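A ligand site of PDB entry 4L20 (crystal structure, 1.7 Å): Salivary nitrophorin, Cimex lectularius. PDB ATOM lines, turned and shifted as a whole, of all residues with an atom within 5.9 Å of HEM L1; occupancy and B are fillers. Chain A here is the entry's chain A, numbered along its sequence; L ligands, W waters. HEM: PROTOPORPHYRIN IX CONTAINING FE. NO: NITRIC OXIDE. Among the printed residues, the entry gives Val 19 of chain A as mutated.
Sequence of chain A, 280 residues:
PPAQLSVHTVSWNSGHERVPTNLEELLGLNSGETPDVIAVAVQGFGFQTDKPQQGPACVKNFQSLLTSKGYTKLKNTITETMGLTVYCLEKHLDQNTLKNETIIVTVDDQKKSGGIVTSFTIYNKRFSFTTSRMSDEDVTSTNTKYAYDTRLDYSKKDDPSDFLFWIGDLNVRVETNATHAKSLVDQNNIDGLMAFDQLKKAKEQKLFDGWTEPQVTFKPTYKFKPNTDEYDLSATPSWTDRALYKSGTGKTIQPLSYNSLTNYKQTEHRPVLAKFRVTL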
ATOM      1  N   TRP A  12       8.026 -18.249  -7.750  1.00  0.00           N
ATOM      2  CA  TRP A  12       9.176 -19.029  -7.463  1.00  0.00           C
ATOM      3  C   TRP A  12       8.862 -20.476  -7.443  1.00  0.00           C
ATOM      4  O   TRP A  12       7.936 -20.951  -6.777  1.00  0.00           O
ATOM      5  CB  TRP A  12       9.670 -18.542  -6.135  1.00  0.00           C
ATOM      6  CG  TRP A  12      11.086 -18.927  -5.683  1.00  0.00           C
ATOM      7  CD1 TRP A  12      12.079 -19.549  -6.377  1.00  0.00           C
ATOM      8  CD2 TRP A  12      11.622 -18.642  -4.387  1.00  0.00           C
ATOM      9  NE1 TRP A  12      13.221 -19.633  -5.586  1.00  0.00           N
ATOM     10  CE2 TRP A  12      12.947 -19.125  -4.350  1.00  0.00           C
ATOM     11  CE3 TRP A  12      11.087 -18.020  -3.238  1.00  0.00           C
ATOM     12  CZ2 TRP A  12      13.767 -18.961  -3.207  1.00  0.00           C
ATOM     13  CZ3 TRP A  12      11.882 -17.874  -2.114  1.00  0.00           C
ATOM     14  CH2 TRP A  12      13.199 -18.365  -2.098  1.00  0.00           C
ATOM     15  N   SER A  14      10.049 -22.952  -5.780  1.00  0.00           N
ATOM     16  CA  SER A  14      10.802 -22.903  -4.529  1.00  0.00           C
ATOM     17  C   SER A  14      11.011 -24.301  -3.976  1.00  0.00           C
ATOM     18  O   SER A  14      11.840 -24.464  -3.077  1.00  0.00           O
ATOM     19  CB  SER A  14      10.003 -22.071  -3.536  1.00  0.00           C
ATOM     20  OG  SER A  14       8.719 -22.617  -3.476  1.00  0.00           O
ATOM     21  N   GLY A  15      10.329 -25.290  -4.536  1.00  0.00           N
ATOM     22  CA  GLY A  15      10.502 -26.692  -4.144  1.00  0.00           C
ATOM     23  C   GLY A  15      10.105 -26.888  -2.683  1.00  0.00           C
ATOM     24  O   GLY A  15       8.923 -26.812  -2.361  1.00  0.00           O
ATOM     25  N   HIS A  16      11.102 -27.116  -1.824  1.00  0.00           N
ATOM     26  CA  HIS A  16      10.914 -27.383  -0.372  1.00  0.00           C
ATOM     27  C   HIS A  16      11.382 -26.188   0.506  1.00  0.00           C
ATOM     28  O   HIS A  16      11.247 -26.208   1.749  1.00  0.00           O
ATOM     29  CB  HIS A  16      11.653 -28.691   0.038  1.00  0.00           C
ATOM     30  CG  HIS A  16      11.069 -29.955  -0.566  1.00  0.00           C
ATOM     31  ND1 HIS A  16       9.996 -30.614  -0.009  1.00  0.00           N
ATOM     32  CD2 HIS A  16      11.423 -30.682  -1.661  1.00  0.00           C
ATOM     33  CE1 HIS A  16       9.702 -31.686  -0.732  1.00  0.00           C
ATOM     34  NE2 HIS A  16      10.550 -31.744  -1.748  1.00  0.00           N
ATOM     35  N   GLU A  17      11.876 -25.131  -0.150  1.00  0.00           N
ATOM     36  CA  GLU A  17      12.422 -23.954   0.531  1.00  0.00           C
ATOM     37  C   GLU A  17      11.343 -23.226   1.405  1.00  0.00           C
ATOM     38  O   GLU A  17      10.148 -23.303   1.107  1.00  0.00           O
ATOM     39  CB  GLU A  17      13.023 -23.010  -0.514  1.00  0.00           C
ATOM     40  CG  GLU A  17      13.969 -21.952   0.037  1.00  0.00           C
ATOM     41  CD  GLU A  17      15.159 -22.572   0.743  1.00  0.00           C
ATOM     42  OE1 GLU A  17      15.726 -21.915   1.648  1.00  0.00           O
ATOM     43  OE2 GLU A  17      15.516 -23.730   0.407  1.00  0.00           O
ATOM     44  N   ARG A  18      11.784 -22.549   2.485  1.00  0.00           N
ATOM     45  CA  ARG A  18      10.844 -21.927   3.442  1.00  0.00           C
ATOM     46  C   ARG A  18      10.771 -20.391   3.303  1.00  0.00           C
ATOM     47  O   ARG A  18      11.663 -19.765   2.704  1.00  0.00           O
ATOM     48  CB  ARG A  18      11.228 -22.300   4.889  1.00  0.00           C
ATOM     49  CG  ARG A  18      11.797 -23.706   5.020  1.00  0.00           C
ATOM     50  CD  ARG A  18      11.276 -24.489   6.235  1.00  0.00           C
ATOM     51  NE  ARG A  18      11.910 -25.811   6.332  1.00  0.00           N
ATOM     52  CZ  ARG A  18      11.664 -26.849   5.517  1.00  0.00           C
ATOM     53  NH1 ARG A  18      12.320 -27.995   5.700  1.00  0.00           N
ATOM     54  NH2 ARG A  18      10.786 -26.762   4.522  1.00  0.00           N
ATOM     55  N   VAL A  19       9.707 -19.793   3.847  1.00  0.00           N
ATOM     56  CA  VAL A  19       9.578 -18.332   3.893  1.00  0.00           C
ATOM     57  C   VAL A  19      10.943 -17.674   4.217  1.00  0.00           C
ATOM     58  O   VAL A  19      11.604 -18.077   5.172  1.00  0.00           O
ATOM     59  CB  VAL A  19       8.500 -17.883   4.930  1.00  0.00           C
ATOM     60  CG1 VAL A  19       8.982 -18.054   6.373  1.00  0.00           C
ATOM     61  CG2 VAL A  19       8.069 -16.438   4.679  1.00  0.00           C
ATOM     62  N   PRO A  20      11.414 -16.758   3.352  1.00  0.00           N
ATOM     63  CA  PRO A  20      12.636 -16.003   3.644  1.00  0.00           C
ATOM     64  C   PRO A  20      12.446 -14.916   4.704  1.00  0.00           C
ATOM     65  O   PRO A  20      11.326 -14.468   4.927  1.00  0.00           O
ATOM     66  CB  PRO A  20      12.984 -15.365   2.296  1.00  0.00           C
ATOM     67  CG  PRO A  20      12.300 -16.236   1.275  1.00  0.00           C
ATOM     68  CD  PRO A  20      11.026 -16.681   1.919  1.00  0.00           C
ATOM     69  N   LEU A  26      11.378  -9.765  -1.824  1.00  0.00           N
ATOM     70  CA  LEU A  26      10.613 -10.724  -2.629  1.00  0.00           C
ATOM     71  C   LEU A  26       9.443 -10.040  -3.280  1.00  0.00           C
ATOM     72  O   LEU A  26       9.092 -10.372  -4.417  1.00  0.00           O
ATOM     73  CB  LEU A  26      10.123 -11.874  -1.735  1.00  0.00           C
ATOM     74  CG  LEU A  26       9.537 -13.082  -2.484  1.00  0.00           C
ATOM     75  CD1 LEU A  26      10.638 -13.843  -3.234  1.00  0.00           C
ATOM     76  CD2 LEU A  26       8.782 -14.010  -1.495  1.00  0.00           C
ATOM     77  N   VAL A  40       1.425 -13.701  -5.337  1.00  0.00           N
ATOM     78  CA  VAL A  40       2.516 -14.576  -5.033  1.00  0.00           C
ATOM     79  C   VAL A  40       2.143 -16.019  -5.436  1.00  0.00           C
ATOM     80  O   VAL A  40       1.222 -16.677  -4.865  1.00  0.00           O
ATOM     81  CB  VAL A  40       2.853 -14.566  -3.479  1.00  0.00           C
ATOM     82  CG1 VAL A  40       4.086 -15.367  -3.208  1.00  0.00           C
ATOM     83  CG2 VAL A  40       2.946 -13.178  -2.949  1.00  0.00           C
ATOM     84  N   VAL A  42       3.821 -19.959  -5.988  1.00  0.00           N
ATOM     85  CA  VAL A  42       4.904 -20.937  -5.727  1.00  0.00           C
ATOM     86  C   VAL A  42       4.572 -22.286  -6.388  1.00  0.00           C
ATOM     87  O   VAL A  42       3.393 -22.667  -6.519  1.00  0.00           O
ATOM     88  CB  VAL A  42       5.236 -21.149  -4.235  1.00  0.00           C
ATOM     89  CG1 VAL A  42       5.927 -19.965  -3.671  1.00  0.00           C
ATOM     90  CG2 VAL A  42       4.010 -21.419  -3.433  1.00  0.00           C
ATOM     91  N   PHE A  45       6.540 -29.072  -3.625  1.00  0.00           N
ATOM     92  CA  PHE A  45       6.044 -30.422  -3.276  1.00  0.00           C
ATOM     93  C   PHE A  45       5.587 -30.350  -1.829  1.00  0.00           C
ATOM     94  O   PHE A  45       6.299 -29.833  -0.979  1.00  0.00           O
ATOM     95  CB  PHE A  45       7.146 -31.502  -3.437  1.00  0.00           C
ATOM     96  CG  PHE A  45       7.619 -31.692  -4.854  1.00  0.00           C
ATOM     97  CD1 PHE A  45       8.860 -31.185  -5.273  1.00  0.00           C
ATOM     98  CD2 PHE A  45       6.819 -32.356  -5.815  1.00  0.00           C
ATOM     99  CE1 PHE A  45       9.300 -31.338  -6.594  1.00  0.00           C
ATOM    100  CE2 PHE A  45       7.255 -32.502  -7.146  1.00  0.00           C
ATOM    101  CZ  PHE A  45       8.495 -31.993  -7.536  1.00  0.00           C
ATOM    102  N   GLY A  46       4.374 -30.832  -1.582  1.00  0.00           N
ATOM    103  CA  GLY A  46       3.892 -31.067  -0.220  1.00  0.00           C
ATOM    104  C   GLY A  46       3.314 -29.898   0.530  1.00  0.00           C
ATOM    105  O   GLY A  46       3.412 -29.856   1.764  1.00  0.00           O
ATOM    106  N   PHE A  47       2.716 -28.922  -0.169  1.00  0.00           N
ATOM    107  CA  PHE A  47       2.230 -27.713   0.521  1.00  0.00           C
ATOM    108  C   PHE A  47       0.988 -28.031   1.416  1.00  0.00           C
ATOM    109  O   PHE A  47       0.897 -27.537   2.547  1.00  0.00           O
ATOM    110  CB  PHE A  47       1.847 -26.584  -0.466  1.00  0.00           C
ATOM    111  CG  PHE A  47       2.996 -26.059  -1.311  1.00  0.00           C
ATOM    112  CD1 PHE A  47       2.942 -26.100  -2.684  1.00  0.00           C
ATOM    113  CD2 PHE A  47       4.079 -25.468  -0.728  1.00  0.00           C
ATOM    114  CE1 PHE A  47       3.966 -25.598  -3.451  1.00  0.00           C
ATOM    115  CE2 PHE A  47       5.123 -24.940  -1.476  1.00  0.00           C
ATOM    116  CZ  PHE A  47       5.071 -25.004  -2.857  1.00  0.00           C
ATOM    117  N   GLN A  48       0.053 -28.820   0.884  1.00  0.00           N
ATOM    118  CA  GLN A  48      -1.163 -29.186   1.603  1.00  0.00           C
ATOM    119  C   GLN A  48      -0.805 -30.176   2.719  1.00  0.00           C
ATOM    120  O   GLN A  48      -1.173 -29.994   3.878  1.00  0.00           O
ATOM    121  CB  GLN A  48      -2.198 -29.773   0.639  1.00  0.00           C
ATOM    122  CG  GLN A  48      -3.644 -29.461   0.945  1.00  0.00           C
ATOM    123  CD  GLN A  48      -4.546 -29.705  -0.254  1.00  0.00           C
ATOM    124  OE1 GLN A  48      -4.084 -30.091  -1.324  1.00  0.00           O
ATOM    125  NE2 GLN A  48      -5.843 -29.466  -0.079  1.00  0.00           N
ATOM    126  N   THR A  49      -0.057 -31.223   2.374  1.00  0.00           N
ATOM    127  CA  THR A  49       0.541 -32.112   3.357  1.00  0.00           C
ATOM    128  C   THR A  49       1.703 -31.363   3.960  1.00  0.00           C
ATOM    129  O   THR A  49       2.873 -31.665   3.706  1.00  0.00           O
ATOM    130  CB  THR A  49       1.106 -33.407   2.727  1.00  0.00           C
ATOM    131  OG1 THR A  49       0.108 -34.047   1.949  1.00  0.00           O
ATOM    132  CG2 THR A  49       1.596 -34.364   3.823  1.00  0.00           C
ATOM    133  N   ASP A  50       1.387 -30.367   4.772  1.00  0.00           N
ATOM    134  CA  ASP A  50       2.405 -29.502   5.321  1.00  0.00           C
ATOM    135  C   ASP A  50       3.153 -30.286   6.420  1.00  0.00           C
ATOM    136  O   ASP A  50       2.989 -30.032   7.619  1.00  0.00           O
ATOM    137  CB  ASP A  50       1.736 -28.215   5.799  1.00  0.00           C
ATOM    138  CG  ASP A  50       2.680 -27.263   6.489  1.00  0.00           C
ATOM    139  OD1 ASP A  50       2.156 -26.426   7.248  1.00  0.00           O
ATOM    140  OD2 ASP A  50       3.915 -27.363   6.310  1.00  0.00           O
ATOM    141  N   LYS A  51       3.967 -31.253   5.990  1.00  0.00           N
ATOM    142  CA  LYS A  51       4.777 -32.088   6.895  1.00  0.00           C
ATOM    143  C   LYS A  51       5.814 -31.282   7.680  1.00  0.00           C
ATOM    144  O   LYS A  51       5.982 -31.507   8.877  1.00  0.00           O
ATOM    145  CB  LYS A  51       5.487 -33.223   6.145  1.00  0.00           C
ATOM    146  CG  LYS A  51       4.703 -34.524   6.050  1.00  0.00           C
ATOM    147  CD  LYS A  51       5.605 -35.744   6.206  1.00  0.00           C
ATOM    148  CE  LYS A  51       4.861 -37.059   5.963  1.00  0.00           C
ATOM    149  NZ  LYS A  51       3.866 -37.408   7.018  1.00  0.00           N
ATOM    150  N   PRO A  52       6.534 -30.344   7.010  1.00  0.00           N
ATOM    151  CA  PRO A  52       7.395 -29.443   7.822  1.00  0.00           C
ATOM    152  C   PRO A  52       6.617 -28.475   8.755  1.00  0.00           C
ATOM    153  O   PRO A  52       7.229 -27.854   9.614  1.00  0.00           O
ATOM    154  CB  PRO A  52       8.225 -28.677   6.768  1.00  0.00           C
ATOM    155  CG  PRO A  52       7.504 -28.854   5.468  1.00  0.00           C
ATOM    156  CD  PRO A  52       6.767 -30.167   5.556  1.00  0.00           C
ATOM    157  N   GLN A  53       5.293 -28.359   8.578  1.00  0.00           N
ATOM    158  CA  GLN A  53       4.475 -27.410   9.341  1.00  0.00           C
ATOM    159  C   GLN A  53       5.120 -26.025   9.234  1.00  0.00           C
ATOM    160  O   GLN A  53       5.474 -25.402  10.196  1.00  0.00           O
ATOM    161  CB  GLN A  53       4.270 -27.878  10.789  1.00  0.00           C
ATOM    162  CG  GLN A  53       3.540 -29.221  10.880  1.00  0.00           C
ATOM    163  CD  GLN A  53       4.187 -30.150  11.878  1.00  0.00           C
ATOM    164  OE1 GLN A  53       4.831 -31.144  11.516  1.00  0.00           O
ATOM    165  NE2 GLN A  53       4.045 -29.815  13.161  1.00  0.00           N
ATOM    166  N   GLN A  54       5.307 -25.595   7.999  1.00  0.00           N
ATOM    167  CA  GLN A  54       5.801 -24.281   7.653  1.00  0.00           C
ATOM    168  C   GLN A  54       4.603 -23.350   7.282  1.00  0.00           C
ATOM    169  O   GLN A  54       4.721 -22.139   7.196  1.00  0.00           O
ATOM    170  CB  GLN A  54       6.818 -24.483   6.513  1.00  0.00           C
ATOM    171  CG  GLN A  54       7.278 -23.242   5.771  1.00  0.00           C
ATOM    172  CD  GLN A  54       8.105 -22.321   6.641  1.00  0.00           C
ATOM    173  OE1 GLN A  54       8.644 -22.733   7.684  1.00  0.00           O
ATOM    174  NE2 GLN A  54       8.234 -21.066   6.210  1.00  0.00           N
ATOM    175  N   GLY A  55       3.417 -23.931   7.087  1.00  0.00           N
ATOM    176  CA  GLY A  55       2.226 -23.143   6.778  1.00  0.00           C
ATOM    177  C   GLY A  55       2.023 -22.054   7.817  1.00  0.00           C
ATOM    178  O   GLY A  55       1.799 -20.892   7.474  1.00  0.00           O
ATOM    179  N   PRO A  56       2.131 -22.426   9.105  1.00  0.00           N
ATOM    180  CA  PRO A  56       1.831 -21.394  10.066  1.00  0.00           C
ATOM    181  C   PRO A  56       2.776 -20.205  10.034  1.00  0.00           C
ATOM    182  O   PRO A  56       2.333 -19.104  10.212  1.00  0.00           O
ATOM    183  CB  PRO A  56       1.897 -22.150  11.435  1.00  0.00           C
ATOM    184  CG  PRO A  56       1.576 -23.542  11.100  1.00  0.00           C
ATOM    185  CD  PRO A  56       2.036 -23.787   9.687  1.00  0.00           C
ATOM    186  N   SNC A  58       4.431 -19.068   7.315  1.00  0.00           N
ATOM    187  CA  SNC A  58       4.090 -18.336   6.111  1.00  0.00           C
ATOM    188  CB  SNC A  58       3.537 -19.307   5.042  1.00  0.00           C
ATOM    189  SG  SNC A  58       4.778 -20.312   4.286  1.00  0.00           S
ATOM    190  ND  SNC A  58       5.453 -18.773   3.535  1.00  0.00           N
ATOM    191  OE  SNC A  58       6.452 -18.892   2.859  1.00  0.00           O
ATOM    192  C   SNC A  58       2.981 -17.353   6.421  1.00  0.00           C
ATOM    193  O   SNC A  58       3.047 -16.163   6.084  1.00  0.00           O
ATOM    194  N   VAL A  59       1.962 -17.847   7.116  1.00  0.00           N
ATOM    195  CA  VAL A  59       0.742 -17.010   7.355  1.00  0.00           C
ATOM    196  C   VAL A  59       1.141 -15.910   8.309  1.00  0.00           C
ATOM    197  O   VAL A  59       0.902 -14.736   8.065  1.00  0.00           O
ATOM    198  CB  VAL A  59      -0.495 -17.823   7.880  1.00  0.00           C
ATOM    199  CG1 VAL A  59      -1.637 -16.896   8.304  1.00  0.00           C
ATOM    200  CG2 VAL A  59      -1.020 -18.800   6.812  1.00  0.00           C
ATOM    201  N   PHE A  62       3.775 -13.359   6.414  1.00  0.00           N
ATOM    202  CA  PHE A  62       3.117 -12.585   5.368  1.00  0.00           C
ATOM    203  C   PHE A  62       2.064 -11.682   5.937  1.00  0.00           C
ATOM    204  O   PHE A  62       2.033 -10.507   5.588  1.00  0.00           O
ATOM    205  CB  PHE A  62       2.556 -13.507   4.245  1.00  0.00           C
ATOM    206  CG  PHE A  62       3.567 -13.811   3.183  1.00  0.00           C
ATOM    207  CD1 PHE A  62       4.252 -15.029   3.172  1.00  0.00           C
ATOM    208  CD2 PHE A  62       3.824 -12.897   2.202  1.00  0.00           C
ATOM    209  CE1 PHE A  62       5.191 -15.308   2.217  1.00  0.00           C
ATOM    210  CE2 PHE A  62       4.770 -13.190   1.188  1.00  0.00           C
ATOM    211  CZ  PHE A  62       5.424 -14.376   1.213  1.00  0.00           C
ATOM    212  N   GLN A  63       1.180 -12.216   6.810  1.00  0.00           N
ATOM    213  CA  GLN A  63       0.144 -11.358   7.424  1.00  0.00           C
ATOM    214  C   GLN A  63       0.689 -10.193   8.236  1.00  0.00           C
ATOM    215  O   GLN A  63       0.240  -9.075   8.141  1.00  0.00           O
ATOM    216  CB  GLN A  63      -0.845 -12.196   8.279  1.00  0.00           C
ATOM    217  CG  GLN A  63      -1.794 -13.069   7.471  1.00  0.00           C
ATOM    218  CD  GLN A  63      -2.766 -12.215   6.692  1.00  0.00           C
ATOM    219  OE1 GLN A  63      -3.380 -11.299   7.261  1.00  0.00           O
ATOM    220  NE2 GLN A  63      -2.894 -12.496   5.386  1.00  0.00           N
ATOM    221  N   LEU A  66       2.047  -7.548   5.646  1.00  0.00           N
ATOM    222  CA  LEU A  66       1.151  -6.938   4.677  1.00  0.00           C
ATOM    223  C   LEU A  66      -0.042  -6.242   5.350  1.00  0.00           C
ATOM    224  O   LEU A  66      -0.459  -5.228   4.843  1.00  0.00           O
ATOM    225  CB  LEU A  66       0.712  -7.923   3.582  1.00  0.00           C
ATOM    226  CG  LEU A  66       1.943  -8.420   2.774  1.00  0.00           C
ATOM    227  CD1 LEU A  66       1.437  -9.465   1.742  1.00  0.00           C
ATOM    228  CD2 LEU A  66       2.704  -7.282   2.078  1.00  0.00           C
ATOM    229  N   LYS A  73      -5.721  -9.930   2.416  1.00  0.00           N
ATOM    230  CA  LYS A  73      -5.611 -11.183   1.609  1.00  0.00           C
ATOM    231  C   LYS A  73      -6.975 -11.548   1.020  1.00  0.00           C
ATOM    232  O   LYS A  73      -7.948 -11.868   1.752  1.00  0.00           O
ATOM    233  CB  LYS A  73      -5.102 -12.292   2.478  1.00  0.00           C
ATOM    234  CG  LYS A  73      -4.863 -13.578   1.738  1.00  0.00           C
ATOM    235  CD  LYS A  73      -4.494 -14.727   2.606  1.00  0.00           C
ATOM    236  CE  LYS A  73      -5.671 -15.192   3.395  1.00  0.00           C
ATOM    237  NZ  LYS A  73      -5.082 -16.083   4.418  1.00  0.00           N
ATOM    238  N   ASN A  76      -5.843 -17.282  -0.483  1.00  0.00           N
ATOM    239  CA  ASN A  76      -4.732 -18.223  -0.615  1.00  0.00           C
ATOM    240  C   ASN A  76      -5.320 -19.587  -1.021  1.00  0.00           C
ATOM    241  O   ASN A  76      -6.306 -20.080  -0.395  1.00  0.00           O
ATOM    242  CB  ASN A  76      -3.966 -18.346   0.721  1.00  0.00           C
ATOM    243  CG  ASN A  76      -3.030 -19.566   0.777  1.00  0.00           C
ATOM    244  OD1 ASN A  76      -3.423 -20.644   1.197  1.00  0.00           O
ATOM    245  ND2 ASN A  76      -1.828 -19.439   0.238  1.00  0.00           N
ATOM    246  N   ILE A  78      -3.845 -23.554  -1.877  1.00  0.00           N
ATOM    247  CA  ILE A  78      -2.689 -24.470  -1.920  1.00  0.00           C
ATOM    248  C   ILE A  78      -3.156 -25.861  -2.400  1.00  0.00           C
ATOM    249  O   ILE A  78      -4.320 -26.288  -2.136  1.00  0.00           O
ATOM    250  CB  ILE A  78      -1.893 -24.564  -0.596  1.00  0.00           C
ATOM    251  CG1 ILE A  78      -2.797 -24.941   0.555  1.00  0.00           C
ATOM    252  CG2 ILE A  78      -1.175 -23.242  -0.243  1.00  0.00           C
ATOM    253  CD1 ILE A  78      -2.018 -25.180   1.831  1.00  0.00           C
ATOM    254  N   THR A  85      -1.476 -16.820  -3.794  1.00  0.00           N
ATOM    255  CA  THR A  85      -2.067 -15.833  -2.888  1.00  0.00           C
ATOM    256  C   THR A  85      -2.236 -14.508  -3.604  1.00  0.00           C
ATOM    257  O   THR A  85      -1.311 -14.015  -4.322  1.00  0.00           O
ATOM    258  CB  THR A  85      -1.196 -15.709  -1.629  1.00  0.00           C
ATOM    259  OG1 THR A  85      -0.912 -17.022  -1.162  1.00  0.00           O
ATOM    260  CG2 THR A  85      -1.946 -14.935  -0.569  1.00  0.00           C
ATOM    261  N   TYR A  87      -3.323 -10.449  -2.825  1.00  0.00           N
ATOM    262  CA  TYR A  87      -3.555  -9.372  -1.836  1.00  0.00           C
ATOM    263  C   TYR A  87      -4.018  -8.122  -2.544  1.00  0.00           C
ATOM    264  O   TYR A  87      -3.563  -7.759  -3.636  1.00  0.00           O
ATOM    265  CB  TYR A  87      -2.274  -9.074  -1.043  1.00  0.00           C
ATOM    266  CG  TYR A  87      -1.668 -10.190  -0.251  1.00  0.00           C
ATOM    267  CD1 TYR A  87      -0.653 -11.034  -0.826  1.00  0.00           C
ATOM    268  CD2 TYR A  87      -2.057 -10.445   1.044  1.00  0.00           C
ATOM    269  CE1 TYR A  87      -0.049 -11.978  -0.079  1.00  0.00           C
ATOM    270  CE2 TYR A  87      -1.477 -11.464   1.787  1.00  0.00           C
ATOM    271  CZ  TYR A  87      -0.506 -12.254   1.196  1.00  0.00           C
ATOM    272  OH  TYR A  87       0.097 -13.277   1.869  1.00  0.00           O
HETATM  273  CHA HEM L   1       0.409 -20.112   2.995  1.00  0.00           C
HETATM  274  CHB HEM L   1       3.950 -18.280   0.200  1.00  0.00           C
HETATM  275  CHC HEM L   1       6.463 -22.373   1.080  1.00  0.00           C
HETATM  276  CHD HEM L   1       2.553 -24.403   3.007  1.00  0.00           C
HETATM  277  C1A HEM L   1       1.191 -19.276   2.224  1.00  0.00           C
HETATM  278  C2A HEM L   1       0.835 -17.957   1.905  1.00  0.00           C
HETATM  279  C3A HEM L   1       1.833 -17.452   1.098  1.00  0.00           C
HETATM  280  C4A HEM L   1       2.765 -18.449   0.925  1.00  0.00           C
HETATM  281  CMA HEM L   1       1.986 -16.073   0.446  1.00  0.00           C
HETATM  282  CAA HEM L   1      -0.394 -17.171   2.398  1.00  0.00           C
HETATM  283  CBA HEM L   1       0.022 -16.184   3.543  1.00  0.00           C
HETATM  284  CGA HEM L   1      -1.121 -15.384   4.118  1.00  0.00           C
HETATM  285  O1A HEM L   1      -1.987 -16.009   4.798  1.00  0.00           O
HETATM  286  O2A HEM L   1      -1.190 -14.161   3.884  1.00  0.00           O
HETATM  287  C1B HEM L   1       4.991 -19.235   0.248  1.00  0.00           C
HETATM  288  C2B HEM L   1       6.306 -19.023  -0.266  1.00  0.00           C
HETATM  289  C3B HEM L   1       7.013 -20.190  -0.019  1.00  0.00           C
HETATM  290  C4B HEM L   1       6.114 -21.105   0.684  1.00  0.00           C
HETATM  291  CMB HEM L   1       6.764 -17.776  -0.938  1.00  0.00           C
HETATM  292  CAB HEM L   1       8.412 -20.554  -0.202  1.00  0.00           C
HETATM  293  CBB HEM L   1       9.333 -19.586  -0.035  1.00  0.00           C
HETATM  294  C1C HEM L   1       5.636 -23.314   1.667  1.00  0.00           C
HETATM  295  C2C HEM L   1       6.007 -24.617   2.055  1.00  0.00           C
HETATM  296  C3C HEM L   1       4.876 -25.184   2.603  1.00  0.00           C
HETATM  297  C4C HEM L   1       3.822 -24.228   2.525  1.00  0.00           C
HETATM  298  CMC HEM L   1       7.379 -25.280   1.897  1.00  0.00           C
HETATM  299  CAC HEM L   1       4.744 -26.565   3.095  1.00  0.00           C
HETATM  300  CBC HEM L   1       5.676 -27.504   2.917  1.00  0.00           C
HETATM  301  C1D HEM L   1       1.691 -23.347   3.207  1.00  0.00           C
HETATM  302  C2D HEM L   1       0.428 -23.500   3.988  1.00  0.00           C
HETATM  303  C3D HEM L   1      -0.191 -22.312   4.003  1.00  0.00           C
HETATM  304  C4D HEM L   1       0.731 -21.438   3.213  1.00  0.00           C
HETATM  305  CMD HEM L   1      -0.116 -24.742   4.658  1.00  0.00           C
HETATM  306  CAD HEM L   1      -1.483 -21.967   4.742  1.00  0.00           C
HETATM  307  CBD HEM L   1      -2.772 -22.044   3.960  1.00  0.00           C
HETATM  308  CGD HEM L   1      -3.954 -21.848   4.885  1.00  0.00           C
HETATM  309  O1D HEM L   1      -3.913 -20.934   5.734  1.00  0.00           O
HETATM  310  O2D HEM L   1      -4.939 -22.635   4.802  1.00  0.00           O
HETATM  311  NA  HEM L   1       2.358 -19.608   1.561  1.00  0.00           N
HETATM  312  NB  HEM L   1       4.917 -20.504   0.672  1.00  0.00           N
HETATM  313  NC  HEM L   1       4.312 -23.125   1.875  1.00  0.00           N
HETATM  314  ND  HEM L   1       1.800 -22.100   2.705  1.00  0.00           N
HETATM  315 FE   HEM L   1       3.292 -21.317   1.708  1.00  0.00          FE
HETATM  316  N    NO L   2       2.465 -21.863   0.215  1.00  0.00           N
HETATM  317  O    NO L   2       2.273 -21.169  -0.631  1.00  0.00           O
HETATM  318  O   HOH W   1      -3.292 -18.582   4.101  1.00  0.00           O
HETATM  319  O   HOH W   2      -5.854 -22.293   1.979  1.00  0.00           O
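OE of SNC 58 lies close to a nitrogen (NB) of HEM L1 (3.1 Å).
Residues that only touch HEM L1: Asn 76, Gly 55, Asp 50, Pro 52, Ile 78, Phe 47, Thr 85, Gly 46, Glu 17, Val 42, Val 59, Arg 18, Phe 62, Trp 12, Ser 14, Pro 20, Val 19 and His 16.
Hydrophobic or aromatic side chains that line HEM L1: Trp 12, Pro 20, Val 42, Phe 47, Pro 52, Val 59, Phe 62, Ile 78 and Tyr 87.
22 residues have an atom within 4 Å of HEM L1: Trp 12, Ser 14, His 16, Glu 17, Arg 18, Val 19, Pro 20, Val 42, Gly 46, Phe 47, Asp 50, Pro 52, Gly 55, SNC 58, Val 59, Phe 62, Gln 63, Lys 73, Asn 76, Ile 78, Thr 85 and Tyr 87.
The nearest printed residue that does not touch HEM L1 is Gln 54 (4.2 Å).
O of Val 40 lies within hydrogen-bond range of N of Thr 85 (2.9 Å).
ND2 of Asn 76 sits at hydrogen-bond distance from OG1 of Thr 85, at 2.9 Å.
The side-chain amide nitrogen (NE2) of Gln 54 sits close to the backbone NH (N) of Val 19 (3.1 Å).
N of Gly 55 lies within hydrogen-bond range of OD1 of Asp 50, at 2.8 Å.
O of His 16 is in hydrogen-bond range of NH2 of Arg 18.
The side-chain carboxylate (OD2) of Asp 50 sits at hydrogen-bond distance from the backbone NH (N) of Gln 54 (2.8 Å).
The backbone NH (N) of Gln 53 sits at hydrogen-bond distance from the side-chain carboxylate (OD2) of Asp 50, 2.8 Å away.
Water W1 lies within hydrogen-bond range of an oxygen (O1D) of HEM L1 (2.9 Å) and the side-chain amino group (NZ) of Lys 73 (3.1 Å).
Water W2 lies within hydrogen-bond range of O2D of HEM L1 (3.0 Å) and OD1 of Asn 76 (3.0 Å).
N of NO L2 binds FE of HEM L1 (1.8 Å).
An oxygen (O1A) of HEM L1 is in salt-bridge range of the side-chain amino group (NZ) of Lys 73 (3.1 Å).
The side-chain amide nitrogen of Gln 63 sits at hydrogen-bond distance from an oxygen (O2A) of HEM L1, 2.8 Å away.
The side-chain hydroxyl (OH) of Tyr 87 sits at hydrogen-bond distance from an oxygen (O2A) of HEM L1 (2.5 Å).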
